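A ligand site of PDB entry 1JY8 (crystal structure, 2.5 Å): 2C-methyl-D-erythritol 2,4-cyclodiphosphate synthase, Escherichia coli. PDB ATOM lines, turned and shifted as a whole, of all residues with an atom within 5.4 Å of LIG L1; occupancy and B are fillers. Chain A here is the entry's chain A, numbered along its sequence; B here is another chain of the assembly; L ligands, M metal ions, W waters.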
ATOM      1  N   ALA A 100      18.227 -12.398  -2.296  1.00  0.00           N
ATOM      2  CA  ALA A 100      18.742 -13.561  -3.011  1.00  0.00           C
ATOM      3  C   ALA A 100      18.269 -13.605  -4.462  1.00  0.00           C
ATOM      4  O   ALA A 100      17.122 -13.266  -4.776  1.00  0.00           O
ATOM      5  CB  ALA A 100      18.322 -14.828  -2.295  1.00  0.00           C
ATOM      6  N   GLN A 101      19.180 -14.000  -5.353  1.00  0.00           N
ATOM      7  CA  GLN A 101      18.875 -14.134  -6.773  1.00  0.00           C
ATOM      8  C   GLN A 101      17.994 -15.382  -6.918  1.00  0.00           C
ATOM      9  O   GLN A 101      17.018 -15.416  -7.680  1.00  0.00           O
ATOM     10  CB  GLN A 101      20.187 -14.309  -7.550  1.00  0.00           C
ATOM     11  CG  GLN A 101      20.109 -14.054  -9.052  1.00  0.00           C
ATOM     12  CD  GLN A 101      19.612 -12.662  -9.382  1.00  0.00           C
ATOM     13  OE1 GLN A 101      18.809 -12.486 -10.309  1.00  0.00           O
ATOM     14  NE2 GLN A 101      20.074 -11.665  -8.651  1.00  0.00           N
ATOM     15  N   ALA A 102      18.351 -16.405  -6.141  1.00  0.00           N
ATOM     16  CA  ALA A 102      17.638 -17.671  -6.115  1.00  0.00           C
ATOM     17  C   ALA A 102      18.056 -18.336  -4.811  1.00  0.00           C
ATOM     18  O   ALA A 102      19.140 -18.055  -4.298  1.00  0.00           O
ATOM     19  CB  ALA A 102      18.045 -18.517  -7.289  1.00  0.00           C
ATOM     20  N   PRO A 103      17.247 -19.268  -4.284  1.00  0.00           N
ATOM     21  CA  PRO A 103      15.975 -19.731  -4.851  1.00  0.00           C
ATOM     22  C   PRO A 103      14.824 -18.746  -4.622  1.00  0.00           C
ATOM     23  O   PRO A 103      15.024 -17.670  -4.048  1.00  0.00           O
ATOM     24  CB  PRO A 103      15.760 -21.058  -4.148  1.00  0.00           C
ATOM     25  CG  PRO A 103      16.421 -20.850  -2.791  1.00  0.00           C
ATOM     26  CD  PRO A 103      17.663 -20.106  -3.135  1.00  0.00           C
ATOM     27  N   LYS A 104      13.645 -19.066  -5.134  1.00  0.00           N
ATOM     28  CA  LYS A 104      12.479 -18.208  -4.956  1.00  0.00           C
ATOM     29  C   LYS A 104      12.003 -18.370  -3.516  1.00  0.00           C
ATOM     30  O   LYS A 104      11.759 -19.480  -3.050  1.00  0.00           O
ATOM     31  CB  LYS A 104      11.373 -18.637  -5.925  1.00  0.00           C
ATOM     32  CG  LYS A 104      10.444 -17.527  -6.354  1.00  0.00           C
ATOM     33  CD  LYS A 104      11.191 -16.506  -7.219  1.00  0.00           C
ATOM     34  CE  LYS A 104      10.345 -15.269  -7.536  1.00  0.00           C
ATOM     35  NZ  LYS A 104      11.187 -14.205  -8.196  1.00  0.00           N
ATOM     36  N   MET A 105      11.866 -17.270  -2.794  1.00  0.00           N
ATOM     37  CA  MET A 105      11.453 -17.324  -1.400  1.00  0.00           C
ATOM     38  C   MET A 105       9.967 -17.216  -1.195  1.00  0.00           C
ATOM     39  O   MET A 105       9.431 -17.802  -0.267  1.00  0.00           O
ATOM     40  CB  MET A 105      12.124 -16.207  -0.610  1.00  0.00           C
ATOM     41  CG  MET A 105      13.622 -16.197  -0.684  1.00  0.00           C
ATOM     42  SD  MET A 105      14.321 -17.673   0.038  1.00  0.00           S
ATOM     43  CE  MET A 105      16.051 -17.504  -0.388  1.00  0.00           C
ATOM     44  N   LEU A 106       9.296 -16.502  -2.077  1.00  0.00           N
ATOM     45  CA  LEU A 106       7.858 -16.250  -1.951  1.00  0.00           C
ATOM     46  C   LEU A 106       6.951 -17.402  -1.508  1.00  0.00           C
ATOM     47  O   LEU A 106       6.145 -17.244  -0.589  1.00  0.00           O
ATOM     48  CB  LEU A 106       7.307 -15.588  -3.225  1.00  0.00           C
ATOM     49  CG  LEU A 106       5.876 -15.030  -3.150  1.00  0.00           C
ATOM     50  CD1 LEU A 106       5.719 -14.047  -1.993  1.00  0.00           C
ATOM     51  CD2 LEU A 106       5.527 -14.353  -4.450  1.00  0.00           C
ATOM     52  N   PRO A 107       7.046 -18.570  -2.153  1.00  0.00           N
ATOM     53  CA  PRO A 107       6.183 -19.675  -1.740  1.00  0.00           C
ATOM     54  C   PRO A 107       6.451 -20.215  -0.335  1.00  0.00           C
ATOM     55  O   PRO A 107       5.616 -20.914   0.246  1.00  0.00           O
ATOM     56  CB  PRO A 107       6.451 -20.729  -2.810  1.00  0.00           C
ATOM     57  CG  PRO A 107       7.851 -20.421  -3.256  1.00  0.00           C
ATOM     58  CD  PRO A 107       7.832 -18.931  -3.336  1.00  0.00           C
ATOM     59  N   ILE A 109       7.439 -18.141   2.255  1.00  0.00           N
ATOM     60  CA  ILE A 109       7.220 -17.108   3.239  1.00  0.00           C
ATOM     61  C   ILE A 109       6.123 -17.391   4.277  1.00  0.00           C
ATOM     62  O   ILE A 109       6.329 -17.162   5.473  1.00  0.00           O
ATOM     63  CB  ILE A 109       7.143 -15.746   2.543  1.00  0.00           C
ATOM     64  CG1 ILE A 109       8.582 -15.381   2.111  1.00  0.00           C
ATOM     65  CG2 ILE A 109       6.491 -14.716   3.442  1.00  0.00           C
ATOM     66  CD1 ILE A 109       8.713 -14.247   1.136  1.00  0.00           C
ATOM     67  N   LYS A 130       9.943 -10.678   3.269  1.00  0.00           N
ATOM     68  CA  LYS A 130       9.846 -10.393   1.846  1.00  0.00           C
ATOM     69  C   LYS A 130      11.174 -10.748   1.223  1.00  0.00           C
ATOM     70  O   LYS A 130      12.113 -11.109   1.942  1.00  0.00           O
ATOM     71  CB  LYS A 130       9.512  -8.917   1.609  1.00  0.00           C
ATOM     72  CG  LYS A 130      10.634  -7.948   1.852  1.00  0.00           C
ATOM     73  CD  LYS A 130      10.140  -6.517   1.716  1.00  0.00           C
ATOM     74  CE  LYS A 130       9.388  -6.079   2.958  1.00  0.00           C
ATOM     75  NZ  LYS A 130      10.346  -5.993   4.102  1.00  0.00           N
ATOM     76  N   ALA A 131      11.247 -10.693  -0.100  1.00  0.00           N
ATOM     77  CA  ALA A 131      12.493 -11.028  -0.791  1.00  0.00           C
ATOM     78  C   ALA A 131      12.687 -10.120  -1.994  1.00  0.00           C
ATOM     79  O   ALA A 131      11.750  -9.455  -2.446  1.00  0.00           O
ATOM     80  CB  ALA A 131      12.480 -12.488  -1.219  1.00  0.00           C
ATOM     81  N   THR A 132      13.926 -10.039  -2.453  1.00  0.00           N
ATOM     82  CA  THR A 132      14.294  -9.252  -3.622  1.00  0.00           C
ATOM     83  C   THR A 132      15.630  -9.791  -4.124  1.00  0.00           C
ATOM     84  O   THR A 132      16.370 -10.410  -3.364  1.00  0.00           O
ATOM     85  CB  THR A 132      14.428  -7.749  -3.317  1.00  0.00           C
ATOM     86  OG1 THR A 132      14.556  -7.024  -4.553  1.00  0.00           O
ATOM     87  CG2 THR A 132      15.668  -7.465  -2.464  1.00  0.00           C
ATOM     88  N   THR A 133      15.892  -9.614  -5.407  1.00  0.00           N
ATOM     89  CA  THR A 133      17.151 -10.043  -5.997  1.00  0.00           C
ATOM     90  C   THR A 133      17.896  -8.737  -6.210  1.00  0.00           C
ATOM     91  O   THR A 133      17.303  -7.654  -6.110  1.00  0.00           O
ATOM     92  CB  THR A 133      16.981 -10.686  -7.404  1.00  0.00           C
ATOM     93  OG1 THR A 133      16.585  -9.686  -8.340  1.00  0.00           O
ATOM     94  CG2 THR A 133      15.944 -11.789  -7.411  1.00  0.00           C
ATOM     95  N   THR A 134      19.198  -8.824  -6.482  1.00  0.00           N
ATOM     96  CA  THR A 134      19.965  -7.624  -6.761  1.00  0.00           C
ATOM     97  C   THR A 134      20.216  -7.540  -8.281  1.00  0.00           C
ATOM     98  O   THR A 134      21.214  -6.986  -8.732  1.00  0.00           O
ATOM     99  CB  THR A 134      21.294  -7.626  -5.996  1.00  0.00           C
ATOM    100  OG1 THR A 134      21.925  -8.901  -6.141  1.00  0.00           O
ATOM    101  CG2 THR A 134      21.042  -7.363  -4.527  1.00  0.00           C
ATOM    102  N   GLU A 135      19.281  -8.119  -9.048  1.00  0.00           N
ATOM    103  CA  GLU A 135      19.342  -8.126 -10.519  1.00  0.00           C
ATOM    104  C   GLU A 135      20.673  -8.615 -11.103  1.00  0.00           C
ATOM    105  O   GLU A 135      21.272  -7.952 -11.951  1.00  0.00           O
ATOM    106  CB  GLU A 135      19.008  -6.737 -11.055  1.00  0.00           C
ATOM    107  CG  GLU A 135      17.743  -6.107 -10.479  1.00  0.00           C
ATOM    108  CD  GLU A 135      16.449  -6.665 -11.058  1.00  0.00           C
ATOM    109  OE1 GLU A 135      15.364  -6.327 -10.561  1.00  0.00           O
ATOM    110  OE2 GLU A 135      16.517  -7.435 -12.041  1.00  0.00           O
ATOM    111  N   ASP B   8      16.003  -2.444  -2.580  1.00  0.00           N
ATOM    112  CA  ASP B   8      15.846  -2.767  -4.004  1.00  0.00           C
ATOM    113  C   ASP B   8      17.107  -2.395  -4.794  1.00  0.00           C
ATOM    114  O   ASP B   8      17.918  -1.554  -4.356  1.00  0.00           O
ATOM    115  CB  ASP B   8      14.629  -2.045  -4.577  1.00  0.00           C
ATOM    116  CG  ASP B   8      14.197  -2.608  -5.924  1.00  0.00           C
ATOM    117  OD1 ASP B   8      13.536  -1.870  -6.677  1.00  0.00           O
ATOM    118  OD2 ASP B   8      14.521  -3.772  -6.260  1.00  0.00           O
ATOM    119  N   HIS B  10      18.521  -2.143  -9.159  1.00  0.00           N
ATOM    120  CA  HIS B  10      18.243  -2.193 -10.600  1.00  0.00           C
ATOM    121  C   HIS B  10      19.537  -1.900 -11.338  1.00  0.00           C
ATOM    122  O   HIS B  10      20.355  -1.100 -10.898  1.00  0.00           O
ATOM    123  CB  HIS B  10      17.104  -1.272 -11.023  1.00  0.00           C
ATOM    124  CG  HIS B  10      15.755  -1.826 -10.687  1.00  0.00           C
ATOM    125  ND1 HIS B  10      15.276  -2.993 -11.242  1.00  0.00           N
ATOM    126  CD2 HIS B  10      14.835  -1.440  -9.766  1.00  0.00           C
ATOM    127  CE1 HIS B  10      14.125  -3.302 -10.672  1.00  0.00           C
ATOM    128  NE2 HIS B  10      13.839  -2.379  -9.766  1.00  0.00           N
ATOM    129  N   ASP B  56       5.207  -7.853  -0.026  1.00  0.00           N
ATOM    130  CA  ASP B  56       6.141  -7.042  -0.776  1.00  0.00           C
ATOM    131  C   ASP B  56       5.562  -6.695  -2.155  1.00  0.00           C
ATOM    132  O   ASP B  56       4.548  -7.268  -2.572  1.00  0.00           O
ATOM    133  CB  ASP B  56       7.514  -7.718  -0.890  1.00  0.00           C
ATOM    134  CG  ASP B  56       7.487  -9.012  -1.679  1.00  0.00           C
ATOM    135  OD1 ASP B  56       6.774  -9.080  -2.695  1.00  0.00           O
ATOM    136  OD2 ASP B  56       8.206  -9.965  -1.295  1.00  0.00           O
ATOM    137  N   ILE B  57       6.251  -5.788  -2.853  1.00  0.00           N
ATOM    138  CA  ILE B  57       5.854  -5.285  -4.164  1.00  0.00           C
ATOM    139  C   ILE B  57       5.654  -6.350  -5.228  1.00  0.00           C
ATOM    140  O   ILE B  57       4.691  -6.287  -5.988  1.00  0.00           O
ATOM    141  CB  ILE B  57       6.852  -4.179  -4.648  1.00  0.00           C
ATOM    142  CG1 ILE B  57       6.210  -3.305  -5.698  1.00  0.00           C
ATOM    143  CG2 ILE B  57       8.123  -4.788  -5.219  1.00  0.00           C
ATOM    144  CD1 ILE B  57       7.097  -2.166  -6.103  1.00  0.00           C
ATOM    145  N   GLY B  58       6.525  -7.356  -5.247  1.00  0.00           N
ATOM    146  CA  GLY B  58       6.402  -8.410  -6.247  1.00  0.00           C
ATOM    147  C   GLY B  58       5.165  -9.250  -6.070  1.00  0.00           C
ATOM    148  O   GLY B  58       4.554  -9.718  -7.036  1.00  0.00           O
ATOM    149  N   LYS B  59       4.763  -9.436  -4.821  1.00  0.00           N
ATOM    150  CA  LYS B  59       3.589 -10.219  -4.476  1.00  0.00           C
ATOM    151  C   LYS B  59       2.303  -9.533  -4.956  1.00  0.00           C
ATOM    152  O   LYS B  59       1.390 -10.197  -5.435  1.00  0.00           O
ATOM    153  CB  LYS B  59       3.555 -10.426  -2.963  1.00  0.00           C
ATOM    154  CG  LYS B  59       2.427 -11.280  -2.460  1.00  0.00           C
ATOM    155  CD  LYS B  59       2.225 -10.951  -1.006  1.00  0.00           C
ATOM    156  CE  LYS B  59       1.115 -11.765  -0.391  1.00  0.00           C
ATOM    157  NZ  LYS B  59       0.854 -11.263   0.991  1.00  0.00           N
ATOM    158  N   ASP B  63       6.043  -9.466 -11.698  1.00  0.00           N
ATOM    159  CA  ASP B  63       6.956  -9.208 -12.825  1.00  0.00           C
ATOM    160  C   ASP B  63       6.417  -9.819 -14.102  1.00  0.00           C
ATOM    161  O   ASP B  63       6.721  -9.363 -15.206  1.00  0.00           O
ATOM    162  CB  ASP B  63       8.326  -9.862 -12.543  1.00  0.00           C
ATOM    163  CG  ASP B  63       9.320  -8.901 -11.932  1.00  0.00           C
ATOM    164  OD1 ASP B  63       8.910  -7.895 -11.305  1.00  0.00           O
ATOM    165  OD2 ASP B  63      10.542  -9.136 -12.086  1.00  0.00           O
HETATM  166  O1  LIG L   1      12.491  -7.318  -7.518  1.00  0.00           O
HETATM  167  P1  LIG L   1      12.696  -8.904  -7.985  1.00  0.00           P
HETATM  168  O2  LIG L   1      13.961  -9.465  -7.342  1.00  0.00           O
HETATM  169  O3  LIG L   1      12.792  -9.027  -9.514  1.00  0.00           O
HETATM  170  O4  LIG L   1      11.389  -9.828  -7.509  1.00  0.00           O
HETATM  171  C1  LIG L   1      10.421  -9.348  -6.587  1.00  0.00           C
HETATM  172  C2  LIG L   1       9.573 -10.481  -6.170  1.00  0.00           C
HETATM  173  O5  LIG L   1      10.157 -11.754  -6.407  1.00  0.00           O
HETATM  174  C3  LIG L   1       9.568 -10.352  -4.639  1.00  0.00           C
HETATM  175  O6  LIG L   1       8.218 -10.354  -4.295  1.00  0.00           O
HETATM  176  C4  LIG L   1      10.223 -11.605  -4.101  1.00  0.00           C
HETATM  177  O7  LIG L   1       9.543 -12.229  -2.997  1.00  0.00           O
HETATM  178  C5  LIG L   1      10.217 -12.534  -5.266  1.00  0.00           C
HETATM  179  N1  LIG L   1      11.545 -12.894  -5.028  1.00  0.00           N
HETATM  180  C6  LIG L   1      11.595 -14.146  -4.378  1.00  0.00           C
HETATM  181  N2  LIG L   1      12.773 -14.763  -4.058  1.00  0.00           N
HETATM  182  C7  LIG L   1      13.942 -14.180  -4.357  1.00  0.00           C
HETATM  183  C8  LIG L   1      13.955 -12.940  -4.989  1.00  0.00           C
HETATM  184  C9  LIG L   1      12.741 -12.354  -5.296  1.00  0.00           C
HETATM  185  O8  LIG L   1      10.579 -14.787  -4.061  1.00  0.00           O
HETATM  186  N3  LIG L   1      15.072 -14.806  -4.039  1.00  0.00           N
HETATM  187  C1  LG2 L   2       6.559  -4.558 -11.316  1.00  0.00           C
HETATM  188  C2  LG2 L   2       7.719  -4.658 -10.277  1.00  0.00           C
HETATM  189  O1  LG2 L   2       8.937  -5.000 -11.001  1.00  0.00           O
HETATM  190  P1  LG2 L   2      10.358  -4.359 -11.470  1.00  0.00           P
HETATM  191  O2  LG2 L   2      11.211  -5.397 -12.298  1.00  0.00           O
HETATM  192  O3  LG2 L   2      10.147  -3.007 -12.323  1.00  0.00           O
HETATM  193  P2  LG2 L   2      11.377  -5.381  -9.211  1.00  0.00           P
HETATM  194  O4  LG2 L   2      10.057  -6.182  -8.738  1.00  0.00           O
HETATM  195  O5  LG2 L   2      12.489  -6.354  -9.746  1.00  0.00           O
HETATM  196  O6  LG2 L   2      11.987  -4.466  -8.057  1.00  0.00           O
HETATM  197  C3  LG2 L   2       8.726  -5.959  -8.176  1.00  0.00           C
HETATM  198  C4  LG2 L   2       7.545  -5.799  -9.222  1.00  0.00           C
HETATM  199  O7  LG2 L   2       6.378  -5.589  -8.426  1.00  0.00           O
HETATM  200  C5  LG2 L   2       7.835  -3.277  -9.559  1.00  0.00           C
HETATM  201  O8  LG2 L   2       6.387  -5.809 -12.013  1.00  0.00           O
HETATM  202  O9  LG2 L   2      11.381  -4.356 -10.315  1.00  0.00           O
HETATM  203 ZN    ZN M   1      12.653  -2.645  -8.210  1.00  0.00          ZN
HETATM  204  O   HOH W   1      10.404  -7.465  -3.316  1.00  0.00           O
HETATM  205  O   HOH W   2      15.362  -6.227  -7.927  1.00  0.00           O
HETATM  206  O   HOH W   3      12.209  -5.675  -5.229  1.00  0.00           O
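An oxygen (O6) of LIG L1 sits at hydrogen-bond distance from the side-chain carboxylate (OD1) of Asp 56 of chain B (2.5 Å).
O of Ala 100 sits at hydrogen-bond distance from N3 of LIG L1, 2.7 Å away.
N of Thr 133 lies within hydrogen-bond range of O2 of LIG L1 (2.7 Å).
O2 of LIG L1 is in hydrogen-bond range of OG1 of Thr 133, at 2.8 Å.
O of Pro 103 lies within hydrogen-bond range of N3 of LIG L1 (2.9 Å).
N of Leu 106 lies within hydrogen-bond range of O8 of LIG L1 (2.9 Å).
N of Met 105 is in hydrogen-bond range of N2 of LIG L1, 3.0 Å away.
An oxygen (O5) of LIG L1 is in hydrogen-bond range of the side-chain amino group (NZ) of Lys 104 (3.2 Å).
An oxygen (O8) of LG2 L2 sits close to the side-chain carboxylate (OD1) of Asp 63 of chain B (3.3 Å).
OE1 of Glu 135 lies close to O5 of LG2 L2 (3.0 Å).
The backbone carbonyl oxygen (O) of Ile 57 of chain B is in hydrogen-bond range of an oxygen (O7) of LG2 L2 (3.0 Å).
An oxygen (O6) of LG2 L2 sits close to an oxygen (O1) of LIG L1, 2.9 Å away.
The backbone NH (N) of Ala 131 lies within hydrogen-bond range of the side-chain carboxylate (OD2) of Asp 56 of chain B, at 3.3 Å.
The side-chain carboxylate of Asp 56 of chain B lies within hydrogen-bond range of the backbone NH of Gly 58 of chain B, at 3.1 Å.
The side-chain carboxylate of Asp 56 of chain B sits at hydrogen-bond distance from the backbone NH of Lys 59 of chain B, at 2.9 Å.
The backbone NH (N) of Ala 100 sits at hydrogen-bond distance from the backbone carbonyl oxygen (O) of Thr 132, at 2.9 Å.
The backbone NH of Glu 135 sits at hydrogen-bond distance from the side-chain hydroxyl of Thr 133 (3.2 Å).
The side-chain carboxylate (OE1) of Glu 135 sits close to a ring nitrogen (ND1) of His 10 of chain B (3.4 Å).
The side-chain carboxylate (OD2) of Asp 63 of chain B lies close to an oxygen (O3) of LIG L1, at 3.4 Å.
Ala 131 touches LIG L1.
Thr 132 touches LIG L1 (OG1 to O1, 3.6 Å).
OE1 of Glu 135 touches O3 of LIG L1, 3.9 Å away.
Gly 58 of chain B touches LIG L1 (CA to O6, 3.3 Å).
Lys 59 of chain B touches LIG L1 (N to O6, 3.6 Å).
Within 4 Å of LIG L1: Ala 100, Pro 103, Lys 104, Met 105, Leu 106, Ala 131, Thr 132, Thr 133, Glu 135, Asp 56 of chain B, Gly 58 of chain B, Lys 59 of chain B and Asp 63 of chain B.
The nearest printed residue that does not touch LIG L1 is Gln 101 (4.1 Å).
Water W3 lies within hydrogen-bond range of the side-chain hydroxyl (OG1) of Thr 132 (2.8 Å), an oxygen (O1) of LIG L1 (2.8 Å) and the side-chain carboxylate (OD2) of Asp 8 of chain B (3.2 Å).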
